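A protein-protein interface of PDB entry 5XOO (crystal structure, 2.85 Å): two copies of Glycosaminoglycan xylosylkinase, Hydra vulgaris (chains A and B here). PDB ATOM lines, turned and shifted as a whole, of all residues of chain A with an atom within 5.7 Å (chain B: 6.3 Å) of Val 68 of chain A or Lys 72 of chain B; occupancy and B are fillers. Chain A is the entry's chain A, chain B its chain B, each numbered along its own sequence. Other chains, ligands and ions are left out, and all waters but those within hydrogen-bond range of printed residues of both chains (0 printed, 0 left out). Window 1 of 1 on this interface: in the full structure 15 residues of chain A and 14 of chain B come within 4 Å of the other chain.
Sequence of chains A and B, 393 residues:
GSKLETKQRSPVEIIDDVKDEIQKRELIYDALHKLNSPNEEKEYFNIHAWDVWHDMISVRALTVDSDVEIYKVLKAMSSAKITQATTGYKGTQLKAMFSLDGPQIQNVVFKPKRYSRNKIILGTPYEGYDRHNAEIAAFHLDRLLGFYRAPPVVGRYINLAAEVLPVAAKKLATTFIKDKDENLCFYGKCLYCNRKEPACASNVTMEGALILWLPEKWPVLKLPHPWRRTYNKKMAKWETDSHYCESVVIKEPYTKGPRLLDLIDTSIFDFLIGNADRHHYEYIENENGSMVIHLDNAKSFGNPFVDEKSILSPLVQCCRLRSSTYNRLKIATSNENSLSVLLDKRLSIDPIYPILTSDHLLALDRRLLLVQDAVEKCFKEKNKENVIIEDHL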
ATOM      1  N   PHE A  45     -11.940  17.638 -22.644  1.00  0.00           N
ATOM      2  CA  PHE A  45     -11.467  16.314 -22.261  1.00  0.00           C
ATOM      3  C   PHE A  45     -11.727  16.014 -20.791  1.00  0.00           C
ATOM      4  O   PHE A  45     -11.110  15.114 -20.225  1.00  0.00           O
ATOM      5  CB  PHE A  45      -9.966  16.186 -22.523  1.00  0.00           C
ATOM      6  CG  PHE A  45      -9.592  16.175 -23.973  1.00  0.00           C
ATOM      7  CD1 PHE A  45      -9.955  15.121 -24.788  1.00  0.00           C
ATOM      8  CD2 PHE A  45      -8.860  17.214 -24.517  1.00  0.00           C
ATOM      9  CE1 PHE A  45      -9.602  15.105 -26.122  1.00  0.00           C
ATOM     10  CE2 PHE A  45      -8.504  17.205 -25.849  1.00  0.00           C
ATOM     11  CZ  PHE A  45      -8.876  16.149 -26.652  1.00  0.00           C
ATOM     12  N   SER A  66      -9.785  -1.509 -15.245  1.00  0.00           N
ATOM     13  CA  SER A  66      -9.006  -0.332 -15.601  1.00  0.00           C
ATOM     14  C   SER A  66      -8.467   0.369 -14.363  1.00  0.00           C
ATOM     15  O   SER A  66      -9.235   0.929 -13.575  1.00  0.00           O
ATOM     16  CB  SER A  66      -9.855   0.637 -16.424  1.00  0.00           C
ATOM     17  OG  SER A  66      -9.213   1.891 -16.547  1.00  0.00           O
ATOM     18  N   ASP A  67      -7.147   0.338 -14.180  1.00  0.00           N
ATOM     19  CA  ASP A  67      -6.548   1.077 -13.077  1.00  0.00           C
ATOM     20  C   ASP A  67      -6.709   2.580 -13.257  1.00  0.00           C
ATOM     21  O   ASP A  67      -6.776   3.315 -12.267  1.00  0.00           O
ATOM     22  CB  ASP A  67      -5.071   0.712 -12.936  1.00  0.00           C
ATOM     23  CG  ASP A  67      -4.867  -0.630 -12.260  1.00  0.00           C
ATOM     24  OD1 ASP A  67      -5.834  -1.153 -11.669  1.00  0.00           O
ATOM     25  OD2 ASP A  67      -3.737  -1.160 -12.317  1.00  0.00           O
ATOM     26  N   VAL A  68      -6.766   3.055 -14.502  1.00  0.00           N
ATOM     27  CA  VAL A  68      -6.905   4.487 -14.746  1.00  0.00           C
ATOM     28  C   VAL A  68      -8.258   4.986 -14.256  1.00  0.00           C
ATOM     29  O   VAL A  68      -8.350   6.028 -13.597  1.00  0.00           O
ATOM     30  CB  VAL A  68      -6.694   4.805 -16.235  1.00  0.00           C
ATOM     31  CG1 VAL A  68      -6.895   6.287 -16.489  1.00  0.00           C
ATOM     32  CG2 VAL A  68      -5.307   4.376 -16.667  1.00  0.00           C
ATOM     33  N   GLU A  69      -9.329   4.255 -14.569  1.00  0.00           N
ATOM     34  CA  GLU A  69     -10.651   4.676 -14.121  1.00  0.00           C
ATOM     35  C   GLU A  69     -10.777   4.581 -12.607  1.00  0.00           C
ATOM     36  O   GLU A  69     -11.396   5.445 -11.975  1.00  0.00           O
ATOM     37  CB  GLU A  69     -11.737   3.842 -14.803  1.00  0.00           C
ATOM     38  CG  GLU A  69     -11.716   3.904 -16.322  1.00  0.00           C
ATOM     39  CD  GLU A  69     -12.967   3.311 -16.945  1.00  0.00           C
ATOM     40  OE1 GLU A  69     -13.040   3.233 -18.191  1.00  0.00           O
ATOM     41  OE2 GLU A  69     -13.878   2.918 -16.189  1.00  0.00           O
ATOM     42  N   ILE A  70     -10.185   3.552 -12.005  1.00  0.00           N
ATOM     43  CA  ILE A  70     -10.330   3.352 -10.568  1.00  0.00           C
ATOM     44  C   ILE A  70      -9.477   4.346  -9.789  1.00  0.00           C
ATOM     45  O   ILE A  70      -9.961   4.984  -8.848  1.00  0.00           O
ATOM     46  CB  ILE A  70     -10.000   1.895 -10.197  1.00  0.00           C
ATOM     47  CG1 ILE A  70     -11.246   1.031 -10.371  1.00  0.00           C
ATOM     48  CG2 ILE A  70      -9.495   1.796  -8.773  1.00  0.00           C
ATOM     49  CD1 ILE A  70     -12.362   1.399  -9.421  1.00  0.00           C
ATOM     50  N   TYR A  71      -8.202   4.501 -10.165  1.00  0.00           N
ATOM     51  CA  TYR A  71      -7.359   5.486  -9.490  1.00  0.00           C
ATOM     52  C   TYR A  71      -7.962   6.879  -9.585  1.00  0.00           C
ATOM     53  O   TYR A  71      -7.818   7.686  -8.661  1.00  0.00           O
ATOM     54  CB  TYR A  71      -5.943   5.504 -10.073  1.00  0.00           C
ATOM     55  CG  TYR A  71      -5.068   4.309  -9.742  1.00  0.00           C
ATOM     56  CD1 TYR A  71      -5.615   3.103  -9.328  1.00  0.00           C
ATOM     57  CD2 TYR A  71      -3.683   4.404  -9.823  1.00  0.00           C
ATOM     58  CE1 TYR A  71      -4.806   2.017  -9.029  1.00  0.00           C
ATOM     59  CE2 TYR A  71      -2.868   3.329  -9.526  1.00  0.00           C
ATOM     60  CZ  TYR A  71      -3.433   2.138  -9.129  1.00  0.00           C
ATOM     61  OH  TYR A  71      -2.620   1.066  -8.828  1.00  0.00           O
ATOM     62  N   LYS A  72      -8.642   7.175 -10.692  1.00  0.00           N
ATOM     63  CA  LYS A  72      -9.295   8.468 -10.837  1.00  0.00           C
ATOM     64  C   LYS A  72     -10.375   8.652  -9.783  1.00  0.00           C
ATOM     65  O   LYS A  72     -10.508   9.733  -9.200  1.00  0.00           O
ATOM     66  CB  LYS A  72      -9.880   8.593 -12.240  1.00  0.00           C
ATOM     67  CG  LYS A  72     -10.632   9.873 -12.503  1.00  0.00           C
ATOM     68  CD  LYS A  72     -10.996   9.962 -13.969  1.00  0.00           C
ATOM     69  CE  LYS A  72     -11.431  11.358 -14.343  1.00  0.00           C
ATOM     70  NZ  LYS A  72     -10.311  12.148 -14.924  1.00  0.00           N
ATOM     71  N   VAL A  73     -11.154   7.602  -9.518  1.00  0.00           N
ATOM     72  CA  VAL A  73     -12.198   7.694  -8.507  1.00  0.00           C
ATOM     73  C   VAL A  73     -11.585   7.757  -7.114  1.00  0.00           C
ATOM     74  O   VAL A  73     -12.001   8.562  -6.275  1.00  0.00           O
ATOM     75  CB  VAL A  73     -13.181   6.518  -8.647  1.00  0.00           C
ATOM     76  CG1 VAL A  73     -14.251   6.591  -7.580  1.00  0.00           C
ATOM     77  CG2 VAL A  73     -13.810   6.519 -10.024  1.00  0.00           C
ATOM     78  N   ILE B  47      -1.290   8.361 -12.216  1.00  0.00           N
ATOM     79  CA  ILE B  47      -0.769   7.639 -13.370  1.00  0.00           C
ATOM     80  C   ILE B  47      -0.515   8.657 -14.466  1.00  0.00           C
ATOM     81  O   ILE B  47      -1.382   9.489 -14.756  1.00  0.00           O
ATOM     82  CB  ILE B  47      -1.734   6.552 -13.875  1.00  0.00           C
ATOM     83  CG1 ILE B  47      -2.294   5.724 -12.724  1.00  0.00           C
ATOM     84  CG2 ILE B  47      -1.028   5.651 -14.867  1.00  0.00           C
ATOM     85  CD1 ILE B  47      -3.197   4.600 -13.194  1.00  0.00           C
ATOM     86  N   HIS B  48       0.667   8.598 -15.072  1.00  0.00           N
ATOM     87  CA  HIS B  48       0.981   9.501 -16.165  1.00  0.00           C
ATOM     88  C   HIS B  48       0.445   8.946 -17.477  1.00  0.00           C
ATOM     89  O   HIS B  48       0.357   7.732 -17.674  1.00  0.00           O
ATOM     90  CB  HIS B  48       2.488   9.726 -16.274  1.00  0.00           C
ATOM     91  CG  HIS B  48       2.859  10.882 -17.152  1.00  0.00           C
ATOM     92  ND1 HIS B  48       2.406  12.162 -16.922  1.00  0.00           N
ATOM     93  CD2 HIS B  48       3.633  10.950 -18.259  1.00  0.00           C
ATOM     94  CE1 HIS B  48       2.886  12.970 -17.849  1.00  0.00           C
ATOM     95  NE2 HIS B  48       3.634  12.259 -18.673  1.00  0.00           N
ATOM     96  N   ALA B  49       0.096   9.860 -18.383  1.00  0.00           N
ATOM     97  CA  ALA B  49      -0.569   9.458 -19.616  1.00  0.00           C
ATOM     98  C   ALA B  49       0.335   8.601 -20.490  1.00  0.00           C
ATOM     99  O   ALA B  49      -0.132   7.656 -21.134  1.00  0.00           O
ATOM    100  CB  ALA B  49      -1.042  10.690 -20.379  1.00  0.00           C
ATOM    101  N   TRP B  50       1.632   8.910 -20.535  1.00  0.00           N
ATOM    102  CA  TRP B  50       2.527   8.092 -21.345  1.00  0.00           C
ATOM    103  C   TRP B  50       2.643   6.682 -20.786  1.00  0.00           C
ATOM    104  O   TRP B  50       2.897   5.737 -21.539  1.00  0.00           O
ATOM    105  CB  TRP B  50       3.909   8.742 -21.445  1.00  0.00           C
ATOM    106  CG  TRP B  50       3.932  10.218 -21.801  1.00  0.00           C
ATOM    107  CD1 TRP B  50       4.879  11.123 -21.416  1.00  0.00           C
ATOM    108  CD2 TRP B  50       2.985  10.953 -22.600  1.00  0.00           C
ATOM    109  NE1 TRP B  50       4.585  12.363 -21.917  1.00  0.00           N
ATOM    110  CE2 TRP B  50       3.429  12.288 -22.646  1.00  0.00           C
ATOM    111  CE3 TRP B  50       1.808  10.614 -23.278  1.00  0.00           C
ATOM    112  CZ2 TRP B  50       2.743  13.279 -23.338  1.00  0.00           C
ATOM    113  CZ3 TRP B  50       1.129  11.599 -23.959  1.00  0.00           C
ATOM    114  CH2 TRP B  50       1.597  12.915 -23.986  1.00  0.00           C
ATOM    115  N   VAL B  52      -0.026   5.242 -19.249  1.00  0.00           N
ATOM    116  CA  VAL B  52      -1.294   4.714 -19.741  1.00  0.00           C
ATOM    117  C   VAL B  52      -1.139   4.217 -21.171  1.00  0.00           C
ATOM    118  O   VAL B  52      -1.636   3.144 -21.529  1.00  0.00           O
ATOM    119  CB  VAL B  52      -2.393   5.785 -19.634  1.00  0.00           C
ATOM    120  CG1 VAL B  52      -3.697   5.278 -20.223  1.00  0.00           C
ATOM    121  CG2 VAL B  52      -2.581   6.209 -18.195  1.00  0.00           C
ATOM    122  N   SER B  66     -12.238   2.377 -23.354  1.00  0.00           N
ATOM    123  CA  SER B  66     -12.406   3.312 -22.250  1.00  0.00           C
ATOM    124  C   SER B  66     -12.185   4.752 -22.694  1.00  0.00           C
ATOM    125  O   SER B  66     -11.068   5.131 -23.054  1.00  0.00           O
ATOM    126  CB  SER B  66     -11.444   2.968 -21.112  1.00  0.00           C
ATOM    127  OG  SER B  66     -11.397   4.010 -20.154  1.00  0.00           O
ATOM    128  N   ASP B  67     -13.249   5.559 -22.676  1.00  0.00           N
ATOM    129  CA  ASP B  67     -13.093   6.975 -22.985  1.00  0.00           C
ATOM    130  C   ASP B  67     -12.239   7.680 -21.943  1.00  0.00           C
ATOM    131  O   ASP B  67     -11.545   8.649 -22.263  1.00  0.00           O
ATOM    132  CB  ASP B  67     -14.459   7.652 -23.089  1.00  0.00           C
ATOM    133  CG  ASP B  67     -15.155   7.365 -24.403  1.00  0.00           C
ATOM    134  OD1 ASP B  67     -14.492   6.870 -25.337  1.00  0.00           O
ATOM    135  OD2 ASP B  67     -16.368   7.645 -24.503  1.00  0.00           O
ATOM    136  N   VAL B  68     -12.271   7.208 -20.697  1.00  0.00           N
ATOM    137  CA  VAL B  68     -11.481   7.836 -19.643  1.00  0.00           C
ATOM    138  C   VAL B  68      -9.996   7.672 -19.927  1.00  0.00           C
ATOM    139  O   VAL B  68      -9.216   8.621 -19.804  1.00  0.00           O
ATOM    140  CB  VAL B  68     -11.860   7.254 -18.271  1.00  0.00           C
ATOM    141  CG1 VAL B  68     -11.004   7.872 -17.182  1.00  0.00           C
ATOM    142  CG2 VAL B  68     -13.334   7.478 -17.993  1.00  0.00           C
ATOM    143  N   GLU B  69      -9.581   6.462 -20.312  1.00  0.00           N
ATOM    144  CA  GLU B  69      -8.175   6.236 -20.625  1.00  0.00           C
ATOM    145  C   GLU B  69      -7.760   6.989 -21.882  1.00  0.00           C
ATOM    146  O   GLU B  69      -6.652   7.530 -21.949  1.00  0.00           O
ATOM    147  CB  GLU B  69      -7.896   4.742 -20.788  1.00  0.00           C
ATOM    148  CG  GLU B  69      -8.235   3.893 -19.582  1.00  0.00           C
ATOM    149  CD  GLU B  69      -7.667   2.489 -19.685  1.00  0.00           C
ATOM    150  OE1 GLU B  69      -7.938   1.665 -18.787  1.00  0.00           O
ATOM    151  OE2 GLU B  69      -6.950   2.207 -20.666  1.00  0.00           O
ATOM    152  N   ILE B  70      -8.639   7.047 -22.881  1.00  0.00           N
ATOM    153  CA  ILE B  70      -8.280   7.675 -24.148  1.00  0.00           C
ATOM    154  C   ILE B  70      -8.257   9.194 -24.006  1.00  0.00           C
ATOM    155  O   ILE B  70      -7.302   9.854 -24.431  1.00  0.00           O
ATOM    156  CB  ILE B  70      -9.238   7.218 -25.262  1.00  0.00           C
ATOM    157  CG1 ILE B  70      -8.749   5.905 -25.864  1.00  0.00           C
ATOM    158  CG2 ILE B  70      -9.348   8.267 -26.347  1.00  0.00           C
ATOM    159  CD1 ILE B  70      -7.429   6.032 -26.588  1.00  0.00           C
ATOM    160  N   TYR B  71      -9.305   9.769 -23.410  1.00  0.00           N
ATOM    161  CA  TYR B  71      -9.330  11.213 -23.196  1.00  0.00           C
ATOM    162  C   TYR B  71      -8.145  11.679 -22.362  1.00  0.00           C
ATOM    163  O   TYR B  71      -7.637  12.787 -22.567  1.00  0.00           O
ATOM    164  CB  TYR B  71     -10.639  11.630 -22.524  1.00  0.00           C
ATOM    165  CG  TYR B  71     -11.868  11.576 -23.412  1.00  0.00           C
ATOM    166  CD1 TYR B  71     -11.878  10.837 -24.587  1.00  0.00           C
ATOM    167  CD2 TYR B  71     -13.021  12.272 -23.070  1.00  0.00           C
ATOM    168  CE1 TYR B  71     -13.001  10.791 -25.392  1.00  0.00           C
ATOM    169  CE2 TYR B  71     -14.147  12.232 -23.870  1.00  0.00           C
ATOM    170  CZ  TYR B  71     -14.130  11.491 -25.029  1.00  0.00           C
ATOM    171  OH  TYR B  71     -15.249  11.446 -25.830  1.00  0.00           O
ATOM    172  N   LYS B  72      -7.696  10.854 -21.417  1.00  0.00           N
ATOM    173  CA  LYS B  72      -6.530  11.210 -20.615  1.00  0.00           C
ATOM    174  C   LYS B  72      -5.283  11.329 -21.477  1.00  0.00           C
ATOM    175  O   LYS B  72      -4.478  12.249 -21.296  1.00  0.00           O
ATOM    176  CB  LYS B  72      -6.323  10.172 -19.516  1.00  0.00           C
ATOM    177  CG  LYS B  72      -5.088  10.396 -18.674  1.00  0.00           C
ATOM    178  CD  LYS B  72      -5.051   9.441 -17.499  1.00  0.00           C
ATOM    179  CE  LYS B  72      -4.023   9.878 -16.483  1.00  0.00           C
ATOM    180  NZ  LYS B  72      -4.651  10.675 -15.401  1.00  0.00           N
ATOM    181  N   VAL B  73      -5.102  10.405 -22.420  1.00  0.00           N
ATOM    182  CA  VAL B  73      -3.935  10.451 -23.289  1.00  0.00           C
ATOM    183  C   VAL B  73      -4.041  11.612 -24.269  1.00  0.00           C
ATOM    184  O   VAL B  73      -3.064  12.333 -24.504  1.00  0.00           O
ATOM    185  CB  VAL B  73      -3.762   9.103 -24.014  1.00  0.00           C
ATOM    186  CG1 VAL B  73      -2.573   9.149 -24.943  1.00  0.00           C
ATOM    187  CG2 VAL B  73      -3.592   7.986 -23.009  1.00  0.00           C
ATOM    188  N   LEU B  74      -5.222  11.814 -24.855  1.00  0.00           N
ATOM    189  CA  LEU B  74      -5.399  12.906 -25.805  1.00  0.00           C
ATOM    190  C   LEU B  74      -5.138  14.258 -25.152  1.00  0.00           C
ATOM    191  O   LEU B  74      -4.415  15.095 -25.702  1.00  0.00           O
ATOM    192  CB  LEU B  74      -6.804  12.860 -26.403  1.00  0.00           C
ATOM    193  CG  LEU B  74      -7.169  11.646 -27.258  1.00  0.00           C
ATOM    194  CD1 LEU B  74      -8.636  11.694 -27.639  1.00  0.00           C
ATOM    195  CD2 LEU B  74      -6.315  11.587 -28.500  1.00  0.00           C
ATOM    196  N   LYS B  75      -5.712  14.485 -23.969  1.00  0.00           N
ATOM    197  CA  LYS B  75      -5.509  15.762 -23.293  1.00  0.00           C
ATOM    198  C   LYS B  75      -4.037  16.009 -22.993  1.00  0.00           C
ATOM    199  O   LYS B  75      -3.587  17.160 -23.006  1.00  0.00           O
ATOM    200  CB  LYS B  75      -6.334  15.829 -22.008  1.00  0.00           C
ATOM    201  CG  LYS B  75      -6.099  17.101 -21.210  1.00  0.00           C
ATOM    202  CD  LYS B  75      -7.120  17.303 -20.107  1.00  0.00           C
ATOM    203  CE  LYS B  75      -7.131  18.757 -19.654  1.00  0.00           C
ATOM    204  NZ  LYS B  75      -8.230  19.051 -18.695  1.00  0.00           N
ATOM    205  N   ALA B  76      -3.271  14.950 -22.729  1.00  0.00           N
ATOM    206  CA  ALA B  76      -1.845  15.130 -22.488  1.00  0.00           C
ATOM    207  C   ALA B  76      -1.126  15.589 -23.747  1.00  0.00           C
ATOM    208  O   ALA B  76      -0.294  16.500 -23.692  1.00  0.00           O
ATOM    209  CB  ALA B  76      -1.227  13.838 -21.963  1.00  0.00           C
ATOM    210  N   MET B  77      -1.431  14.977 -24.893  1.00  0.00           N
ATOM    211  CA  MET B  77      -0.805  15.412 -26.136  1.00  0.00           C
ATOM    212  C   MET B  77      -1.174  16.850 -26.469  1.00  0.00           C
ATOM    213  O   MET B  77      -0.348  17.602 -26.997  1.00  0.00           O
ATOM    214  CB  MET B  77      -1.188  14.494 -27.294  1.00  0.00           C
ATOM    215  CG  MET B  77      -0.823  13.041 -27.125  1.00  0.00           C
ATOM    216  SD  MET B  77      -1.413  12.079 -28.527  1.00  0.00           S
ATOM    217  CE  MET B  77      -2.875  11.366 -27.816  1.00  0.00           C
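The side-chain hydroxyl (OG) of Ser 66 of chain B is in hydrogen-bond range of the side-chain carboxylate (OE1) of Glu 69 of chain A, 2.7 Å away.
The side-chain carboxylate (OE1) of Glu 69 of chain B sits at hydrogen-bond distance from the side-chain hydroxyl (OG) of Ser 66 of chain A (2.6 Å).
The side-chain hydroxyl (OG) of Ser 66 of chain B sits at hydrogen-bond distance from the backbone NH (N) of Glu 69 of chain B, at 3.1 Å.
The side-chain hydroxyl of Ser 66 of chain A lies close to the backbone NH of Val 68 of chain A (3.4 Å).
The side-chain hydroxyl (OG) of Ser 66 of chain B sits close to the backbone NH (N) of Val 68 of chain B (3.4 Å).
OG of Ser 66 of chain A is in hydrogen-bond range of N of Glu 69 of chain A, 3.1 Å away.
Among the printed residues, merely in contact across the chains: Phe 45 of chain A with Tyr 71 of chain B (3.97 Å), Phe 45 of chain A with Leu 74 of chain B (3.6 Å), Phe 45 of chain A with Lys 75 of chain B (3.7 Å), Asp 67 of chain A with Ile 47 of chain B (3.9 Å), Val 68 of chain A with Val 52 of chain B (3.6 Å), Val 68 of chain A with Glu 69 of chain B (3.8 Å), Val 68 of chain A with Lys 72 of chain B (3.8 Å), Glu 69 of chain A with Val 68 of chain B (3.9 Å), Tyr 71 of chain A with Ile 47 of chain B (3.4 Å) and Lys 72 of chain A with Val 68 of chain B (3.8 Å).
Printed residues of chain B within 4 Å of Phe 45 of chain A: Tyr 71, Leu 74 and Lys 75.
Val 68 of chain A touches just these residues of chain B: Val 52, Glu 69 and Lys 72.
Printed residues of chain B within 4 Å of Lys 72 of chain A: Val 68.
Of the printed residues of chain A, Val 52 of chain B touches Val 68.
Of the printed residues of chain A, Val 68 of chain B touches Glu 69 (3.9 Å) and Lys 72 (3.8 Å).
Of chain A, only Val 68 comes within 4 Å of Lys 72 of chain B.
The nearest residue of chain B that does not touch Val 68 of chain A is Ile 47 of chain B (4.02 Å).
The nearest printed residue of chain A that does not touch Lys 75 of chain B is Lys 72 of chain A (8.0 Å).
Hydrophobic or aromatic side chains of chain B within 4 Å of the printed part of chain A: Ile 47, Val 52, Val 68 and Leu 74.
Of the 9 printed residues of chain A, 7 touch a printed residue of chain B.
Printed residues of chain A that touch a printed residue of chain B: Phe 45, Ser 66, Asp 67, Val 68, Glu 69, Tyr 71 and Lys 72.
Hydrophobic or aromatic side chains of chain A that line the printed part of chain B: Phe 45, Val 68 and Tyr 71.
Along chain A the printed residues that touch a printed residue of chain B span positions 45 to 72.
Among the printed residues, no Asp or Glu carboxylate lies within 4 Å of a Lys or Arg side-chain nitrogen of the other chain.
Ser 66 of chain A touches Glu 69 of chain B, and with the chains exchanged Glu 69 of chain A touches Ser 66 of chain B.
Val 68 of chain A touches Glu 69 of chain B, and with the chains exchanged Glu 69 of chain A touches Val 68 of chain B.
Val 68 of chain A touches Lys 72 of chain B, and with the chains exchanged Lys 72 of chain A touches Val 68 of chain B.
Positions printed for both chains: 66, 67, 68, 69, 70, 71, 72 and 73.
Of the 12 pairs that touch across the chains among the printed residues, 6 have their exchanged pair printed and touching as well.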
